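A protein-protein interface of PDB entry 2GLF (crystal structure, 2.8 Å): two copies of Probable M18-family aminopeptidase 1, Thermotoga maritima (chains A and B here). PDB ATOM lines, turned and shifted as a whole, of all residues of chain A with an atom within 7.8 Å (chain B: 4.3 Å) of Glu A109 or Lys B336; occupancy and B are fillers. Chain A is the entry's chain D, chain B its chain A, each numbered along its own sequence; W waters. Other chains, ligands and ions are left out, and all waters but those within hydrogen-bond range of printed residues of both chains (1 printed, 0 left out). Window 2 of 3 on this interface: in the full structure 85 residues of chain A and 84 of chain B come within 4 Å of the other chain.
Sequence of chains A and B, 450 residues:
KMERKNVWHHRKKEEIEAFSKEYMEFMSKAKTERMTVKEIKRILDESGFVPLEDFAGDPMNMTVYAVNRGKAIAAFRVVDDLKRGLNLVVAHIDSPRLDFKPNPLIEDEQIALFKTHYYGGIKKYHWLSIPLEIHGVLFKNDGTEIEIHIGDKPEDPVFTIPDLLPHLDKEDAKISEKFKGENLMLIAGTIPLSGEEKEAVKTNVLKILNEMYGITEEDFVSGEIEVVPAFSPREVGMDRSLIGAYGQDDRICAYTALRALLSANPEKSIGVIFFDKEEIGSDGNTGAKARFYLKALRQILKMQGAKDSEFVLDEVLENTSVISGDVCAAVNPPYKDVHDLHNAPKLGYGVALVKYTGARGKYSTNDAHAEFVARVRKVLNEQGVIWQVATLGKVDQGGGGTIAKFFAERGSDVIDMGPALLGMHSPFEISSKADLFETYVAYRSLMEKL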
ATOM      1  N   ILE A 106      -2.148  10.560  15.610  1.00  0.00           N
ATOM      2  CA  ILE A 106      -3.228  10.003  16.414  1.00  0.00           C
ATOM      3  C   ILE A 106      -2.669   8.825  17.196  1.00  0.00           C
ATOM      4  O   ILE A 106      -1.561   8.359  16.924  1.00  0.00           O
ATOM      5  CB  ILE A 106      -4.390   9.442  15.568  1.00  0.00           C
ATOM      6  CG1 ILE A 106      -3.950   8.142  14.883  1.00  0.00           C
ATOM      7  CG2 ILE A 106      -4.867  10.483  14.569  1.00  0.00           C
ATOM      8  CD1 ILE A 106      -5.100   7.209  14.533  1.00  0.00           C
ATOM      9  N   GLU A 107      -3.448   8.347  18.164  1.00  0.00           N
ATOM     10  CA  GLU A 107      -3.059   7.195  18.956  1.00  0.00           C
ATOM     11  C   GLU A 107      -4.240   6.244  18.971  1.00  0.00           C
ATOM     12  O   GLU A 107      -5.377   6.662  19.191  1.00  0.00           O
ATOM     13  CB  GLU A 107      -2.697   7.588  20.391  1.00  0.00           C
ATOM     14  CG  GLU A 107      -2.077   6.429  21.179  1.00  0.00           C
ATOM     15  CD  GLU A 107      -1.809   6.748  22.646  1.00  0.00           C
ATOM     16  OE1 GLU A 107      -1.039   7.695  22.939  1.00  0.00           O
ATOM     17  OE2 GLU A 107      -2.370   6.039  23.514  1.00  0.00           O
ATOM     18  N   ASP A 108      -3.970   4.969  18.718  1.00  0.00           N
ATOM     19  CA  ASP A 108      -5.014   3.946  18.711  1.00  0.00           C
ATOM     20  C   ASP A 108      -4.441   2.684  19.341  1.00  0.00           C
ATOM     21  O   ASP A 108      -3.543   2.055  18.780  1.00  0.00           O
ATOM     22  CB  ASP A 108      -5.467   3.649  17.276  1.00  0.00           C
ATOM     23  CG  ASP A 108      -6.746   2.825  17.221  1.00  0.00           C
ATOM     24  OD1 ASP A 108      -7.106   2.352  16.121  1.00  0.00           O
ATOM     25  OD2 ASP A 108      -7.396   2.658  18.273  1.00  0.00           O
ATOM     26  N   GLU A 109      -4.956   2.318  20.509  1.00  0.00           N
ATOM     27  CA  GLU A 109      -4.471   1.131  21.203  1.00  0.00           C
ATOM     28  C   GLU A 109      -3.020   1.314  21.651  1.00  0.00           C
ATOM     29  O   GLU A 109      -2.199   0.416  21.485  1.00  0.00           O
ATOM     30  CB  GLU A 109      -4.587  -0.094  20.292  1.00  0.00           C
ATOM     31  CG  GLU A 109      -6.013  -0.534  20.013  1.00  0.00           C
ATOM     32  CD  GLU A 109      -6.732  -0.995  21.270  1.00  0.00           C
ATOM     33  OE1 GLU A 109      -6.246  -1.941  21.933  1.00  0.00           O
ATOM     34  OE2 GLU A 109      -7.788  -0.410  21.597  1.00  0.00           O
ATOM     35  N   GLN A 110      -2.714   2.486  22.209  1.00  0.00           N
ATOM     36  CA  GLN A 110      -1.372   2.814  22.704  1.00  0.00           C
ATOM     37  C   GLN A 110      -0.283   2.805  21.636  1.00  0.00           C
ATOM     38  O   GLN A 110       0.873   2.493  21.916  1.00  0.00           O
ATOM     39  CB  GLN A 110      -0.972   1.857  23.835  1.00  0.00           C
ATOM     40  CG  GLN A 110      -1.804   1.984  25.107  1.00  0.00           C
ATOM     41  CD  GLN A 110      -3.263   1.637  24.893  1.00  0.00           C
ATOM     42  OE1 GLN A 110      -3.591   0.546  24.432  1.00  0.00           O
ATOM     43  NE2 GLN A 110      -4.149   2.566  25.231  1.00  0.00           N
ATOM     44  N   ILE A 111      -0.653   3.145  20.409  1.00  0.00           N
ATOM     45  CA  ILE A 111       0.309   3.182  19.318  1.00  0.00           C
ATOM     46  C   ILE A 111       0.140   4.457  18.510  1.00  0.00           C
ATOM     47  O   ILE A 111      -0.890   4.666  17.877  1.00  0.00           O
ATOM     48  CB  ILE A 111       0.138   1.968  18.378  1.00  0.00           C
ATOM     49  CG1 ILE A 111       0.620   0.700  19.084  1.00  0.00           C
ATOM     50  CG2 ILE A 111       0.919   2.183  17.087  1.00  0.00           C
ATOM     51  CD1 ILE A 111       0.540  -0.538  18.216  1.00  0.00           C
ATOM     52  N   ALA A 112       1.155   5.313  18.540  1.00  0.00           N
ATOM     53  CA  ALA A 112       1.103   6.559  17.787  1.00  0.00           C
ATOM     54  C   ALA A 112       1.115   6.233  16.291  1.00  0.00           C
ATOM     55  O   ALA A 112       1.933   5.440  15.819  1.00  0.00           O
ATOM     56  CB  ALA A 112       2.300   7.453  18.152  1.00  0.00           C
ATOM     57  N   LEU A 113       0.202   6.847  15.548  1.00  0.00           N
ATOM     58  CA  LEU A 113       0.110   6.611  14.113  1.00  0.00           C
ATOM     59  C   LEU A 113       0.062   7.909  13.324  1.00  0.00           C
ATOM     60  O   LEU A 113      -0.423   8.929  13.804  1.00  0.00           O
ATOM     61  CB  LEU A 113      -1.138   5.785  13.803  1.00  0.00           C
ATOM     62  CG  LEU A 113      -1.163   4.393  14.431  1.00  0.00           C
ATOM     63  CD1 LEU A 113      -2.582   3.865  14.475  1.00  0.00           C
ATOM     64  CD2 LEU A 113      -0.256   3.472  13.633  1.00  0.00           C
ATOM     65  N   LEU A 164      -1.384  -7.234   7.989  1.00  0.00           N
ATOM     66  CA  LEU A 164      -1.922  -8.149   8.978  1.00  0.00           C
ATOM     67  C   LEU A 164      -1.340  -9.520   8.672  1.00  0.00           C
ATOM     68  O   LEU A 164      -1.256  -9.906   7.509  1.00  0.00           O
ATOM     69  CB  LEU A 164      -3.445  -8.189   8.870  1.00  0.00           C
ATOM     70  CG  LEU A 164      -4.171  -9.272   9.667  1.00  0.00           C
ATOM     71  CD1 LEU A 164      -3.927  -9.089  11.151  1.00  0.00           C
ATOM     72  CD2 LEU A 164      -5.659  -9.200   9.356  1.00  0.00           C
ATOM     73  N   THR A 190       4.671   3.918  19.961  1.00  0.00           N
ATOM     74  CA  THR A 190       4.600   2.747  20.857  1.00  0.00           C
ATOM     75  C   THR A 190       5.180   2.924  22.268  1.00  0.00           C
ATOM     76  O   THR A 190       4.755   2.221  23.189  1.00  0.00           O
ATOM     77  CB  THR A 190       5.240   1.446  20.262  1.00  0.00           C
ATOM     78  OG1 THR A 190       6.607   1.338  20.675  1.00  0.00           O
ATOM     79  CG2 THR A 190       5.157   1.438  18.750  1.00  0.00           C
ATOM     80  N   VAL A 201       1.621   7.701  24.624  1.00  0.00           N
ATOM     81  CA  VAL A 201       2.484   7.441  23.479  1.00  0.00           C
ATOM     82  C   VAL A 201       2.450   8.577  22.465  1.00  0.00           C
ATOM     83  O   VAL A 201       3.490   8.964  21.928  1.00  0.00           O
ATOM     84  CB  VAL A 201       2.107   6.107  22.799  1.00  0.00           C
ATOM     85  CG1 VAL A 201       2.962   5.879  21.567  1.00  0.00           C
ATOM     86  CG2 VAL A 201       2.306   4.967  23.780  1.00  0.00           C
ATOM     87  N   ASN B 332      -2.679  -5.033  15.836  1.00  0.00           N
ATOM     88  CA  ASN B 332      -2.403  -4.113  14.744  1.00  0.00           C
ATOM     89  C   ASN B 332      -3.644  -3.219  14.740  1.00  0.00           C
ATOM     90  O   ASN B 332      -4.663  -3.557  14.143  1.00  0.00           O
ATOM     91  CB  ASN B 332      -2.288  -4.918  13.452  1.00  0.00           C
ATOM     92  CG  ASN B 332      -1.609  -4.163  12.349  1.00  0.00           C
ATOM     93  OD1 ASN B 332      -0.859  -4.744  11.573  1.00  0.00           O
ATOM     94  ND2 ASN B 332      -1.873  -2.871  12.256  1.00  0.00           N
ATOM     95  N   PRO B 333      -3.567  -2.060  15.411  1.00  0.00           N
ATOM     96  CA  PRO B 333      -4.676  -1.107  15.516  1.00  0.00           C
ATOM     97  C   PRO B 333      -5.779  -1.168  14.446  1.00  0.00           C
ATOM     98  O   PRO B 333      -6.913  -1.553  14.743  1.00  0.00           O
ATOM     99  CB  PRO B 333      -3.960   0.236  15.573  1.00  0.00           C
ATOM    100  CG  PRO B 333      -2.754  -0.094  16.355  1.00  0.00           C
ATOM    101  CD  PRO B 333      -2.290  -1.394  15.734  1.00  0.00           C
ATOM    102  N   PRO B 334      -5.466  -0.803  13.190  1.00  0.00           N
ATOM    103  CA  PRO B 334      -6.500  -0.846  12.146  1.00  0.00           C
ATOM    104  C   PRO B 334      -7.245  -2.175  12.031  1.00  0.00           C
ATOM    105  O   PRO B 334      -8.377  -2.215  11.542  1.00  0.00           O
ATOM    106  CB  PRO B 334      -5.723  -0.511  10.875  1.00  0.00           C
ATOM    107  CG  PRO B 334      -4.343  -1.039  11.176  1.00  0.00           C
ATOM    108  CD  PRO B 334      -4.138  -0.572  12.596  1.00  0.00           C
ATOM    109  N   TYR B 335      -6.608  -3.254  12.481  1.00  0.00           N
ATOM    110  CA  TYR B 335      -7.203  -4.582  12.416  1.00  0.00           C
ATOM    111  C   TYR B 335      -7.376  -5.194  13.799  1.00  0.00           C
ATOM    112  O   TYR B 335      -7.334  -6.415  13.958  1.00  0.00           O
ATOM    113  CB  TYR B 335      -6.339  -5.498  11.555  1.00  0.00           C
ATOM    114  CG  TYR B 335      -5.841  -4.839  10.294  1.00  0.00           C
ATOM    115  CD1 TYR B 335      -4.509  -4.449  10.174  1.00  0.00           C
ATOM    116  CD2 TYR B 335      -6.700  -4.589   9.223  1.00  0.00           C
ATOM    117  CE1 TYR B 335      -4.041  -3.828   9.019  1.00  0.00           C
ATOM    118  CE2 TYR B 335      -6.243  -3.969   8.062  1.00  0.00           C
ATOM    119  CZ  TYR B 335      -4.913  -3.591   7.967  1.00  0.00           C
ATOM    120  OH  TYR B 335      -4.442  -2.972   6.829  1.00  0.00           O
ATOM    121  N   LYS B 336      -7.584  -4.337  14.793  1.00  0.00           N
ATOM    122  CA  LYS B 336      -7.765  -4.785  16.170  1.00  0.00           C
ATOM    123  C   LYS B 336      -8.955  -5.746  16.343  1.00  0.00           C
ATOM    124  O   LYS B 336      -8.982  -6.526  17.287  1.00  0.00           O
ATOM    125  CB  LYS B 336      -7.944  -3.576  17.104  1.00  0.00           C
ATOM    126  CG  LYS B 336      -9.363  -3.036  17.143  1.00  0.00           C
ATOM    127  CD  LYS B 336      -9.556  -1.959  18.200  1.00  0.00           C
ATOM    128  CE  LYS B 336      -8.922  -0.637  17.791  1.00  0.00           C
ATOM    129  NZ  LYS B 336      -9.316   0.487  18.696  1.00  0.00           N
ATOM    130  N   ASP B 337      -9.936  -5.694  15.446  1.00  0.00           N
ATOM    131  CA  ASP B 337     -11.092  -6.582  15.566  1.00  0.00           C
ATOM    132  C   ASP B 337     -10.785  -8.054  15.305  1.00  0.00           C
ATOM    133  O   ASP B 337     -11.669  -8.911  15.383  1.00  0.00           O
ATOM    134  CB  ASP B 337     -12.216  -6.145  14.627  1.00  0.00           C
ATOM    135  CG  ASP B 337     -13.180  -5.184  15.289  1.00  0.00           C
ATOM    136  OD1 ASP B 337     -14.248  -4.917  14.698  1.00  0.00           O
ATOM    137  OD2 ASP B 337     -12.873  -4.692  16.397  1.00  0.00           O
ATOM    138  N   VAL B 338      -9.531  -8.350  15.002  1.00  0.00           N
ATOM    139  CA  VAL B 338      -9.126  -9.715  14.712  1.00  0.00           C
ATOM    140  C   VAL B 338      -8.693 -10.447  16.003  1.00  0.00           C
ATOM    141  O   VAL B 338      -8.464 -11.660  16.011  1.00  0.00           O
ATOM    142  CB  VAL B 338      -7.976  -9.671  13.681  1.00  0.00           C
ATOM    143  CG1 VAL B 338      -6.627  -9.842  14.375  1.00  0.00           C
ATOM    144  CG2 VAL B 338      -8.203 -10.701  12.614  1.00  0.00           C
ATOM    145  N   HIS B 339      -8.612  -9.683  17.091  1.00  0.00           N
ATOM    146  CA  HIS B 339      -8.183 -10.173  18.398  1.00  0.00           C
ATOM    147  C   HIS B 339      -9.215  -9.999  19.491  1.00  0.00           C
ATOM    148  O   HIS B 339     -10.209  -9.290  19.330  1.00  0.00           O
ATOM    149  CB  HIS B 339      -6.949  -9.404  18.878  1.00  0.00           C
ATOM    150  CG  HIS B 339      -5.652  -9.901  18.329  1.00  0.00           C
ATOM    151  ND1 HIS B 339      -5.172 -11.167  18.585  1.00  0.00           N
ATOM    152  CD2 HIS B 339      -4.714  -9.288  17.570  1.00  0.00           C
ATOM    153  CE1 HIS B 339      -3.993 -11.312  18.009  1.00  0.00           C
ATOM    154  NE2 HIS B 339      -3.692 -10.187  17.387  1.00  0.00           N
ATOM    155  N   LEU B 341      -8.999  -8.378  22.644  1.00  0.00           N
ATOM    156  CA  LEU B 341      -8.150  -7.439  23.358  1.00  0.00           C
ATOM    157  C   LEU B 341      -7.768  -7.842  24.777  1.00  0.00           C
ATOM    158  O   LEU B 341      -6.657  -7.553  25.215  1.00  0.00           O
ATOM    159  CB  LEU B 341      -8.783  -6.042  23.374  1.00  0.00           C
ATOM    160  CG  LEU B 341      -8.778  -5.188  22.095  1.00  0.00           C
ATOM    161  CD1 LEU B 341      -7.524  -5.448  21.283  1.00  0.00           C
ATOM    162  CD2 LEU B 341      -9.993  -5.512  21.264  1.00  0.00           C
ATOM    163  N   LYS B 346       0.461  -6.736  23.465  1.00  0.00           N
ATOM    164  CA  LYS B 346       0.704  -5.378  22.987  1.00  0.00           C
ATOM    165  C   LYS B 346       2.223  -5.204  22.911  1.00  0.00           C
ATOM    166  O   LYS B 346       2.956  -5.756  23.743  1.00  0.00           O
ATOM    167  CB  LYS B 346       0.127  -4.353  23.970  1.00  0.00           C
ATOM    168  CG  LYS B 346      -1.350  -4.500  24.264  1.00  0.00           C
ATOM    169  CD  LYS B 346      -2.205  -4.059  23.092  1.00  0.00           C
ATOM    170  CE  LYS B 346      -3.259  -3.062  23.547  1.00  0.00           C
ATOM    171  NZ  LYS B 346      -2.608  -1.874  24.153  1.00  0.00           N
HETATM  172  O   HOH W   1      -0.568  -1.953  21.747  1.00  0.00           O
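Of the 10 printed residues of chain B, 4 touch a printed residue of chain A.
Printed residues of chain B that touch a printed residue of chain A: Pro B333, Lys B336, Leu B341 and Lys B346.
Hydrophobic or aromatic side chains of chain B within 4 Å of the printed part of chain A: Pro B333 and Leu B341.
Among the printed residues, Asp or Glu carboxylates within 4 Å of a Lys or Arg side-chain nitrogen of the other chain: Asp A108 with Lys B336 (2.9 Å) and Glu A109 with Lys B336 (3.4 Å).
Among the printed residues, pairs that only touch across the chains: Asp A108 with Pro B333, Glu A109 with Lys B346, Glu A109 with Leu B341 and Ile A111 with Pro B333.
Water W1 lies within hydrogen-bond range of O of Glu A109 (2.9 Å) and NZ of Lys B346 (3.2 Å).
No position is printed for both chains.
Of the 7 pairs that touch across the chains among the printed residues, none has its exchanged pair printed and touching as well.
Of the printed residues of chain B, Asp A108 touches Pro B333 and Lys B336.
Of chain B, only Lys B336, Leu B341 and Lys B346 come within 4 Å of Glu A109.
Of the printed residues of chain B, Gln A110 touches Lys B346.
Of the printed residues of chain B, Ile A111 touches Pro B333 (3.8 Å).
Of chain A, only Asp A108 and Glu A109 come within 4 Å of Lys B336.
Printed residues of chain A within 4 Å of Lys B346: Glu A109 and Gln A110.
The nearest printed residue of chain B that does not touch Glu A109 is Pro B333 (4.3 Å).
The nearest residue of chain A that does not touch Lys B336 is Leu A164 (7.0 Å).
The nearest printed residue of chain A that does not touch Lys B346 is Ile A111 (6.5 Å).
The side-chain amino group (NZ) of Lys B336 lies within salt-bridge range of the side-chain carboxylate (OE2) of Glu A109.
NZ of Lys B336 lies within salt-bridge range of OD2 of Asp A108 (2.9 Å).
The side-chain amino group (NZ) of Lys B346 sits at hydrogen-bond distance from the side-chain amide oxygen (OE1) of Gln A110.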
